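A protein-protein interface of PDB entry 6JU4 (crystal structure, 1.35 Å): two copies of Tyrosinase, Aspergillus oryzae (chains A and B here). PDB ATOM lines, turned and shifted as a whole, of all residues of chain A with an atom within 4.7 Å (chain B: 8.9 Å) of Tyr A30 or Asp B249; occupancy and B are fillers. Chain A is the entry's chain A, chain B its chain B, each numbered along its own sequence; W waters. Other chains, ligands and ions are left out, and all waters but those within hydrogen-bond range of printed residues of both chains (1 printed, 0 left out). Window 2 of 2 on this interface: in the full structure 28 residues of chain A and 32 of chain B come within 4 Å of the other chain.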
ATOM      1  N   ILE A  26      -1.645  -5.131  -6.341  1.00  0.00           N
ATOM      2  CA  ILE A  26      -1.946  -3.696  -6.429  1.00  0.00           C
ATOM      3  C   ILE A  26      -3.145  -3.388  -7.304  1.00  0.00           C
ATOM      4  O   ILE A  26      -3.817  -2.358  -7.111  1.00  0.00           O
ATOM      5  CB  ILE A  26      -0.705  -2.916  -6.924  1.00  0.00           C
ATOM      6  CG1 ILE A  26      -0.909  -1.405  -6.738  1.00  0.00           C
ATOM      7  CG2 ILE A  26      -0.334  -3.284  -8.345  1.00  0.00           C
ATOM      8  CD1 ILE A  26       0.329  -0.566  -6.975  1.00  0.00           C
ATOM      9  N   ASP A  27      -3.428  -4.236  -8.300  1.00  0.00           N
ATOM     10  CA  ASP A  27      -4.652  -4.024  -9.092  1.00  0.00           C
ATOM     11  C   ASP A  27      -5.895  -4.368  -8.284  1.00  0.00           C
ATOM     12  O   ASP A  27      -6.907  -3.654  -8.334  1.00  0.00           O
ATOM     13  CB  ASP A  27      -4.592  -4.857 -10.368  1.00  0.00           C
ATOM     14  CG  ASP A  27      -3.830  -4.196 -11.497  1.00  0.00           C
ATOM     15  OD1 ASP A  27      -3.299  -3.075 -11.309  1.00  0.00           O
ATOM     16  OD2 ASP A  27      -3.719  -4.842 -12.565  1.00  0.00           O
ATOM     17  N   ASP A  28      -5.884  -5.476  -7.540  1.00  0.00           N
ATOM     18  CA  ASP A  28      -7.002  -5.795  -6.661  1.00  0.00           C
ATOM     19  C   ASP A  28      -7.240  -4.705  -5.625  1.00  0.00           C
ATOM     20  O   ASP A  28      -8.361  -4.272  -5.369  1.00  0.00           O
ATOM     21  CB  ASP A  28      -6.713  -7.101  -5.901  1.00  0.00           C
ATOM     22  CG  ASP A  28      -6.706  -8.367  -6.723  1.00  0.00           C
ATOM     23  OD1 ASP A  28      -7.145  -8.360  -7.889  1.00  0.00           O
ATOM     24  OD2 ASP A  28      -6.266  -9.403  -6.179  1.00  0.00           O
ATOM     25  N   TRP A  29      -6.136  -4.261  -5.008  1.00  0.00           N
ATOM     26  CA  TRP A  29      -6.211  -3.202  -3.999  1.00  0.00           C
ATOM     27  C   TRP A  29      -6.750  -1.911  -4.607  1.00  0.00           C
ATOM     28  O   TRP A  29      -7.629  -1.260  -4.040  1.00  0.00           O
ATOM     29  CB  TRP A  29      -4.821  -2.998  -3.407  1.00  0.00           C
ATOM     30  CG  TRP A  29      -4.652  -1.874  -2.440  1.00  0.00           C
ATOM     31  CD1 TRP A  29      -4.993  -1.871  -1.108  1.00  0.00           C
ATOM     32  CD2 TRP A  29      -4.095  -0.585  -2.725  1.00  0.00           C
ATOM     33  NE1 TRP A  29      -4.683  -0.659  -0.560  1.00  0.00           N
ATOM     34  CE2 TRP A  29      -4.125   0.143  -1.523  1.00  0.00           C
ATOM     35  CE3 TRP A  29      -3.553   0.014  -3.877  1.00  0.00           C
ATOM     36  CZ2 TRP A  29      -3.652   1.448  -1.429  1.00  0.00           C
ATOM     37  CZ3 TRP A  29      -3.087   1.312  -3.781  1.00  0.00           C
ATOM     38  CH2 TRP A  29      -3.134   2.022  -2.566  1.00  0.00           C
ATOM     39  N   TYR A  30      -6.234  -1.496  -5.775  1.00  0.00           N
ATOM     40  CA  TYR A  30      -6.734  -0.284  -6.413  1.00  0.00           C
ATOM     41  C   TYR A  30      -8.237  -0.380  -6.683  1.00  0.00           C
ATOM     42  O   TYR A  30      -8.998   0.566  -6.453  1.00  0.00           O
ATOM     43  CB  TYR A  30      -5.929  -0.003  -7.707  1.00  0.00           C
ATOM     44  CG  TYR A  30      -6.483   1.250  -8.363  1.00  0.00           C
ATOM     45  CD1 TYR A  30      -6.154   2.495  -7.829  1.00  0.00           C
ATOM     46  CD2 TYR A  30      -7.339   1.205  -9.458  1.00  0.00           C
ATOM     47  CE1 TYR A  30      -6.636   3.658  -8.382  1.00  0.00           C
ATOM     48  CE2 TYR A  30      -7.844   2.374 -10.023  1.00  0.00           C
ATOM     49  CZ  TYR A  30      -7.480   3.587  -9.482  1.00  0.00           C
ATOM     50  OH  TYR A  30      -7.975   4.772  -9.978  1.00  0.00           O
ATOM     51  N   LEU A  31      -8.702  -1.530  -7.167  1.00  0.00           N
ATOM     52  CA  LEU A  31     -10.133  -1.695  -7.433  1.00  0.00           C
ATOM     53  C   LEU A  31     -10.953  -1.673  -6.158  1.00  0.00           C
ATOM     54  O   LEU A  31     -12.041  -1.050  -6.127  1.00  0.00           O
ATOM     55  CB  LEU A  31     -10.363  -2.963  -8.274  1.00  0.00           C
ATOM     56  CG  LEU A  31      -9.705  -2.893  -9.669  1.00  0.00           C
ATOM     57  CD1 LEU A  31      -9.640  -4.266 -10.322  1.00  0.00           C
ATOM     58  CD2 LEU A  31     -10.425  -1.904 -10.571  1.00  0.00           C
ATOM     59  N   GLU A  32     -10.462  -2.270  -5.070  1.00  0.00           N
ATOM     60  CA  GLU A  32     -11.139  -2.184  -3.771  1.00  0.00           C
ATOM     61  C   GLU A  32     -11.237  -0.729  -3.314  1.00  0.00           C
ATOM     62  O   GLU A  32     -12.247  -0.285  -2.785  1.00  0.00           O
ATOM     63  CB  GLU A  32     -10.413  -2.961  -2.663  1.00  0.00           C
ATOM     64  CG  GLU A  32     -10.000  -4.376  -2.906  1.00  0.00           C
ATOM     65  CD  GLU A  32      -9.306  -5.071  -1.748  1.00  0.00           C
ATOM     66  OE1 GLU A  32      -9.609  -6.255  -1.519  1.00  0.00           O
ATOM     67  OE2 GLU A  32      -8.450  -4.480  -1.052  1.00  0.00           O
ATOM     68  N   GLN A  33     -10.139   0.008  -3.494  1.00  0.00           N
ATOM     69  CA  GLN A  33     -10.070   1.377  -2.989  1.00  0.00           C
ATOM     70  C   GLN A  33     -10.992   2.310  -3.765  1.00  0.00           C
ATOM     71  O   GLN A  33     -11.458   3.317  -3.251  1.00  0.00           O
ATOM     72  CB  GLN A  33      -8.617   1.864  -3.052  1.00  0.00           C
ATOM     73  CG  GLN A  33      -7.763   1.261  -1.937  1.00  0.00           C
ATOM     74  CD  GLN A  33      -8.094   1.801  -0.555  1.00  0.00           C
ATOM     75  OE1 GLN A  33      -8.081   3.016  -0.305  1.00  0.00           O
ATOM     76  NE2 GLN A  33      -8.371   0.862   0.370  1.00  0.00           N
ATOM     77  N   THR A  34     -11.259   2.015  -5.032  1.00  0.00           N
ATOM     78  CA  THR A  34     -11.930   2.994  -5.883  1.00  0.00           C
ATOM     79  C   THR A  34     -13.309   2.563  -6.324  1.00  0.00           C
ATOM     80  O   THR A  34     -13.980   3.325  -7.024  1.00  0.00           O
ATOM     81  CB  THR A  34     -11.090   3.258  -7.158  1.00  0.00           C
ATOM     82  OG1 THR A  34     -10.854   2.030  -7.870  1.00  0.00           O
ATOM     83  CG2 THR A  34      -9.755   3.852  -6.784  1.00  0.00           C
ATOM     84  N   LEU A  43      -5.608   4.391  -0.249  1.00  0.00           N
ATOM     85  CA  LEU A  43      -5.052   4.980  -1.472  1.00  0.00           C
ATOM     86  C   LEU A  43      -4.585   6.400  -1.193  1.00  0.00           C
ATOM     87  O   LEU A  43      -3.504   6.811  -1.601  1.00  0.00           O
ATOM     88  CB  LEU A  43      -6.107   4.972  -2.589  1.00  0.00           C
ATOM     89  CG  LEU A  43      -5.693   5.557  -3.932  1.00  0.00           C
ATOM     90  CD1 LEU A  43      -4.459   4.867  -4.493  1.00  0.00           C
ATOM     91  CD2 LEU A  43      -6.857   5.416  -4.907  1.00  0.00           C
ATOM     92  N   ILE A 172      -2.552  -0.952 -13.022  1.00  0.00           N
ATOM     93  CA  ILE A 172      -3.438   0.155 -13.381  1.00  0.00           C
ATOM     94  C   ILE A 172      -2.916   1.488 -12.856  1.00  0.00           C
ATOM     95  O   ILE A 172      -2.816   2.482 -13.569  1.00  0.00           O
ATOM     96  CB  ILE A 172      -4.846  -0.092 -12.801  1.00  0.00           C
ATOM     97  CG1 ILE A 172      -5.513  -1.339 -13.383  1.00  0.00           C
ATOM     98  CG2 ILE A 172      -5.716   1.146 -13.010  1.00  0.00           C
ATOM     99  CD1 ILE A 172      -6.657  -1.888 -12.563  1.00  0.00           C
ATOM    100  N   LEU A 173      -2.633   1.530 -11.555  1.00  0.00           N
ATOM    101  CA  LEU A 173      -2.263   2.786 -10.897  1.00  0.00           C
ATOM    102  C   LEU A 173      -0.977   3.354 -11.471  1.00  0.00           C
ATOM    103  O   LEU A 173      -0.792   4.583 -11.499  1.00  0.00           O
ATOM    104  CB  LEU A 173      -2.127   2.519  -9.392  1.00  0.00           C
ATOM    105  CG  LEU A 173      -1.957   3.709  -8.455  1.00  0.00           C
ATOM    106  CD1 LEU A 173      -3.010   4.761  -8.724  1.00  0.00           C
ATOM    107  CD2 LEU A 173      -2.005   3.246  -7.002  1.00  0.00           C
ATOM    108  N   MET A 176      -1.503   5.763 -14.540  1.00  0.00           N
ATOM    109  CA  MET A 176      -2.343   6.940 -14.318  1.00  0.00           C
ATOM    110  C   MET A 176      -1.518   8.159 -13.934  1.00  0.00           C
ATOM    111  O   MET A 176      -0.911   8.200 -12.856  1.00  0.00           O
ATOM    112  CB  MET A 176      -3.355   6.664 -13.197  1.00  0.00           C
ATOM    113  CG  MET A 176      -4.368   5.562 -13.562  1.00  0.00           C
ATOM    114  SD  MET A 176      -5.370   5.051 -12.159  1.00  0.00           S
ATOM    115  CE  MET A 176      -5.821   6.636 -11.460  1.00  0.00           C
ATOM    116  N   LEU B 205     -12.938  15.211 -14.016  1.00  0.00           N
ATOM    117  CA  LEU B 205     -13.371  14.696 -15.315  1.00  0.00           C
ATOM    118  C   LEU B 205     -14.263  15.704 -16.027  1.00  0.00           C
ATOM    119  O   LEU B 205     -15.134  16.366 -15.440  1.00  0.00           O
ATOM    120  CB  LEU B 205     -14.088  13.354 -15.171  1.00  0.00           C
ATOM    121  CG  LEU B 205     -13.343  12.266 -14.383  1.00  0.00           C
ATOM    122  CD1 LEU B 205     -14.092  10.945 -14.486  1.00  0.00           C
ATOM    123  CD2 LEU B 205     -11.899  12.126 -14.864  1.00  0.00           C
ATOM    124  N   LYS B 233     -15.079  10.963 -19.628  1.00  0.00           N
ATOM    125  CA  LYS B 233     -14.252  10.366 -18.586  1.00  0.00           C
ATOM    126  C   LYS B 233     -12.811  10.849 -18.628  1.00  0.00           C
ATOM    127  O   LYS B 233     -11.974  10.310 -17.896  1.00  0.00           O
ATOM    128  CB  LYS B 233     -14.284   8.841 -18.716  1.00  0.00           C
ATOM    129  CG  LYS B 233     -15.690   8.289 -18.479  1.00  0.00           C
ATOM    130  CD  LYS B 233     -15.729   6.777 -18.601  1.00  0.00           C
ATOM    131  CE  LYS B 233     -17.144   6.237 -18.474  1.00  0.00           C
ATOM    132  NZ  LYS B 233     -17.513   5.366 -19.631  1.00  0.00           N
ATOM    133  N   CYS B 234     -12.504  11.868 -19.428  1.00  0.00           N
ATOM    134  CA  CYS B 234     -11.172  12.461 -19.480  1.00  0.00           C
ATOM    135  C   CYS B 234     -11.090  13.714 -18.608  1.00  0.00           C
ATOM    136  O   CYS B 234     -11.996  14.553 -18.711  1.00  0.00           O
ATOM    137  CB  CYS B 234     -10.840  12.901 -20.920  1.00  0.00           C
ATOM    138  SG  CYS B 234     -10.858  11.509 -22.086  1.00  0.00           S
ATOM    139  N   GLN B 235     -10.012  13.857 -17.850  1.00  0.00           N
ATOM    140  CA  GLN B 235      -9.657  15.112 -17.180  1.00  0.00           C
ATOM    141  C   GLN B 235      -8.668  15.910 -18.029  1.00  0.00           C
ATOM    142  O   GLN B 235      -8.684  17.149 -18.012  1.00  0.00           O
ATOM    143  CB  GLN B 235      -9.080  14.772 -15.796  1.00  0.00           C
ATOM    144  CG  GLN B 235      -8.462  15.904 -15.004  1.00  0.00           C
ATOM    145  CD  GLN B 235      -7.788  15.426 -13.723  1.00  0.00           C
ATOM    146  OE1 GLN B 235      -7.688  14.214 -13.432  1.00  0.00           O
ATOM    147  NE2 GLN B 235      -7.280  16.363 -12.937  1.00  0.00           N
ATOM    148  N   SER B 236      -7.822  15.209 -18.784  1.00  0.00           N
ATOM    149  CA  SER B 236      -6.850  15.825 -19.671  1.00  0.00           C
ATOM    150  C   SER B 236      -7.052  15.367 -21.110  1.00  0.00           C
ATOM    151  O   SER B 236      -7.580  14.289 -21.395  1.00  0.00           O
ATOM    152  CB  SER B 236      -5.419  15.437 -19.242  1.00  0.00           C
ATOM    153  OG  SER B 236      -5.089  16.245 -18.124  1.00  0.00           O
ATOM    154  N   GLY B 241      -4.543   7.867 -26.369  1.00  0.00           N
ATOM    155  CA  GLY B 241      -4.605   7.290 -25.051  1.00  0.00           C
ATOM    156  C   GLY B 241      -5.839   6.512 -24.660  1.00  0.00           C
ATOM    157  O   GLY B 241      -5.824   5.837 -23.621  1.00  0.00           O
ATOM    158  N   LEU B 242      -6.922   6.639 -25.429  1.00  0.00           N
ATOM    159  CA  LEU B 242      -8.181   5.975 -25.080  1.00  0.00           C
ATOM    160  C   LEU B 242      -8.314   4.665 -25.844  1.00  0.00           C
ATOM    161  O   LEU B 242      -8.482   4.640 -27.066  1.00  0.00           O
ATOM    162  CB  LEU B 242      -9.383   6.888 -25.341  1.00  0.00           C
ATOM    163  CG  LEU B 242      -9.244   8.320 -24.811  1.00  0.00           C
ATOM    164  CD1 LEU B 242     -10.455   9.151 -25.223  1.00  0.00           C
ATOM    165  CD2 LEU B 242      -9.080   8.299 -23.293  1.00  0.00           C
ATOM    166  N   TYR B 246      -9.252  -1.144 -20.847  1.00  0.00           N
ATOM    167  CA  TYR B 246      -8.388  -0.669 -19.772  1.00  0.00           C
ATOM    168  C   TYR B 246      -9.276  -0.052 -18.705  1.00  0.00           C
ATOM    169  O   TYR B 246     -10.410   0.310 -19.025  1.00  0.00           O
ATOM    170  CB  TYR B 246      -7.336   0.349 -20.274  1.00  0.00           C
ATOM    171  CG  TYR B 246      -6.398  -0.384 -21.210  1.00  0.00           C
ATOM    172  CD1 TYR B 246      -5.301  -1.084 -20.733  1.00  0.00           C
ATOM    173  CD2 TYR B 246      -6.693  -0.400 -22.572  1.00  0.00           C
ATOM    174  CE1 TYR B 246      -4.478  -1.757 -21.624  1.00  0.00           C
ATOM    175  CE2 TYR B 246      -5.884  -1.074 -23.449  1.00  0.00           C
ATOM    176  CZ  TYR B 246      -4.786  -1.746 -22.963  1.00  0.00           C
ATOM    177  OH  TYR B 246      -3.995  -2.420 -23.859  1.00  0.00           O
ATOM    178  N   ASN B 247      -8.794   0.011 -17.475  1.00  0.00           N
ATOM    179  CA  ASN B 247      -9.600   0.585 -16.398  1.00  0.00           C
ATOM    180  C   ASN B 247     -10.011   2.014 -16.755  1.00  0.00           C
ATOM    181  O   ASN B 247      -9.196   2.787 -17.303  1.00  0.00           O
ATOM    182  CB  ASN B 247      -8.813   0.541 -15.088  1.00  0.00           C
ATOM    183  CG  ASN B 247      -9.597   1.122 -13.944  1.00  0.00           C
ATOM    184  OD1 ASN B 247      -9.694   2.332 -13.756  1.00  0.00           O
ATOM    185  ND2 ASN B 247     -10.141   0.237 -13.110  1.00  0.00           N
ATOM    186  N   ALA B 248     -11.264   2.367 -16.493  1.00  0.00           N
ATOM    187  CA  ALA B 248     -11.774   3.667 -16.897  1.00  0.00           C
ATOM    188  C   ALA B 248     -10.983   4.815 -16.291  1.00  0.00           C
ATOM    189  O   ALA B 248     -10.944   5.923 -16.850  1.00  0.00           O
ATOM    190  CB  ALA B 248     -13.246   3.781 -16.516  1.00  0.00           C
ATOM    191  N   ASP B 249     -10.293   4.589 -15.179  1.00  0.00           N
ATOM    192  CA  ASP B 249      -9.492   5.683 -14.607  1.00  0.00           C
ATOM    193  C   ASP B 249      -8.244   5.959 -15.434  1.00  0.00           C
ATOM    194  O   ASP B 249      -7.658   7.040 -15.306  1.00  0.00           O
ATOM    195  CB  ASP B 249      -9.124   5.399 -13.148  1.00  0.00           C
ATOM    196  CG  ASP B 249     -10.314   5.390 -12.221  1.00  0.00           C
ATOM    197  OD1 ASP B 249     -11.363   5.966 -12.583  1.00  0.00           O
ATOM    198  OD2 ASP B 249     -10.221   4.773 -11.142  1.00  0.00           O
ATOM    199  N   VAL B 250      -7.824   5.026 -16.276  1.00  0.00           N
ATOM    200  CA  VAL B 250      -6.722   5.304 -17.195  1.00  0.00           C
ATOM    201  C   VAL B 250      -7.106   6.392 -18.193  1.00  0.00           C
ATOM    202  O   VAL B 250      -6.291   7.203 -18.635  1.00  0.00           O
ATOM    203  CB  VAL B 250      -6.294   4.013 -17.913  1.00  0.00           C
ATOM    204  CG1 VAL B 250      -5.232   4.275 -18.963  1.00  0.00           C
ATOM    205  CG2 VAL B 250      -5.775   3.037 -16.861  1.00  0.00           C
ATOM    206  N   TRP B 251      -8.393   6.427 -18.544  1.00  0.00           N
ATOM    207  CA  TRP B 251      -8.865   7.436 -19.495  1.00  0.00           C
ATOM    208  C   TRP B 251      -8.885   8.843 -18.912  1.00  0.00           C
ATOM    209  O   TRP B 251      -8.983   9.797 -19.689  1.00  0.00           O
ATOM    210  CB  TRP B 251     -10.261   7.100 -20.019  1.00  0.00           C
ATOM    211  CG  TRP B 251     -10.372   5.719 -20.590  1.00  0.00           C
ATOM    212  CD1 TRP B 251      -9.394   5.010 -21.222  1.00  0.00           C
ATOM    213  CD2 TRP B 251     -11.556   4.905 -20.581  1.00  0.00           C
ATOM    214  NE1 TRP B 251      -9.898   3.778 -21.603  1.00  0.00           N
ATOM    215  CE2 TRP B 251     -11.217   3.692 -21.217  1.00  0.00           C
ATOM    216  CE3 TRP B 251     -12.850   5.075 -20.080  1.00  0.00           C
ATOM    217  CZ2 TRP B 251     -12.156   2.672 -21.362  1.00  0.00           C
ATOM    218  CZ3 TRP B 251     -13.774   4.049 -20.239  1.00  0.00           C
ATOM    219  CH2 TRP B 251     -13.426   2.843 -20.879  1.00  0.00           C
ATOM    220  N   ALA B 252      -8.777   9.001 -17.595  1.00  0.00           N
ATOM    221  CA  ALA B 252      -8.719  10.372 -17.056  1.00  0.00           C
ATOM    222  C   ALA B 252      -7.600  11.155 -17.719  1.00  0.00           C
ATOM    223  O   ALA B 252      -7.724  12.333 -18.050  1.00  0.00           O
ATOM    224  CB  ALA B 252      -8.574  10.326 -15.533  1.00  0.00           C
ATOM    225  N   ASP B 253      -6.464  10.489 -17.918  1.00  0.00           N
ATOM    226  CA  ASP B 253      -5.373  11.115 -18.674  1.00  0.00           C
ATOM    227  C   ASP B 253      -4.629   9.981 -19.366  1.00  0.00           C
ATOM    228  O   ASP B 253      -3.839   9.264 -18.753  1.00  0.00           O
ATOM    229  CB  ASP B 253      -4.437  11.886 -17.748  1.00  0.00           C
ATOM    230  CG  ASP B 253      -3.310  12.570 -18.501  1.00  0.00           C
ATOM    231  OD1 ASP B 253      -2.959  12.169 -19.639  1.00  0.00           O
ATOM    232  OD2 ASP B 253      -2.753  13.543 -17.936  1.00  0.00           O
ATOM    233  N   GLY B 254      -4.940   9.793 -20.643  1.00  0.00           N
ATOM    234  CA  GLY B 254      -4.409   8.656 -21.377  1.00  0.00           C
ATOM    235  C   GLY B 254      -3.021   8.927 -21.900  1.00  0.00           C
ATOM    236  O   GLY B 254      -2.464   8.048 -22.559  1.00  0.00           O
ATOM    237  N   GLY B 255      -2.453  10.102 -21.621  1.00  0.00           N
ATOM    238  CA  GLY B 255      -1.082  10.391 -22.016  1.00  0.00           C
ATOM    239  C   GLY B 255      -0.956  11.005 -23.398  1.00  0.00           C
ATOM    240  O   GLY B 255      -1.910  11.115 -24.172  1.00  0.00           O
HETATM  241  O   HOH W   1     -11.291   1.993 -10.666  1.00  0.00           O
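OD1 of Asp A27 lies within hydrogen-bond range of N of Ile A172 (2.8 Å). The backbone carbonyl oxygen (O) of Tyr A30 sits at hydrogen-bond distance from the side-chain hydroxyl (OG1) of Thr A34, 2.8 Å away. The side-chain hydroxyl (OH) of Tyr A30 sits close to the side-chain sulfur (SD) of Met A176 (3.4 Å). The backbone NH (N) of Asp B249 is in hydrogen-bond range of the side-chain amide oxygen (OD1) of Asn B247 (2.7 Å).
Of the 13 printed residues of chain A, 4 touch a printed residue of chain B. Along chain A the printed residues that touch a printed residue of chain B span positions 30 to 176. Of the 17 printed residues of chain B, 2 touch a printed residue of chain A. Among the printed residues, 4 pairs touch across the chains. Among the printed residues, no Asp or Glu carboxylate lies within 4 Å of a Lys or Arg side-chain nitrogen of the other chain.
Tyr A30 touches just one residue of chain B: Asp B249 (2.5 Å). Asp B249 touches two residues of chain A. Of the printed residues of chain A, Asn B247 touches Leu A31 (3.3 Å) and Ile A172 (3.8 Å). Printed residues of chain B within 4 Å of Ile A172: Asn B247. Of the printed residues of chain B, Leu A31 touches Asn B247. Of the printed residues of chain B, Met A176 touches Asp B249. Ala B248 touches none of the printed residues of chain A. Ile A26 touches none of the printed residues of chain B. The nearest printed residue of chain B that does not touch Met A176 is Val B250 (4.3 Å).
Water W1 lies within hydrogen-bond range of the side-chain hydroxyl of Thr A34, the side-chain carboxylate of Asp B249 and the side-chain amide nitrogen of Asn B247.
CD2 of Leu A31 touches ND2 of Asn B247 (3.3 Å). Ile A172 touches Asn B247 (CG2 to CB, 3.8 Å). Met A176 touches Asp B249.
No position is printed for both chains. Of the 4 pairs that touch across the chains among the printed residues, none has its exchanged pair printed and touching as well.
The side-chain hydroxyl of Tyr A30 sits at hydrogen-bond distance from the side-chain carboxylate of Asp B249 (2.5 Å).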
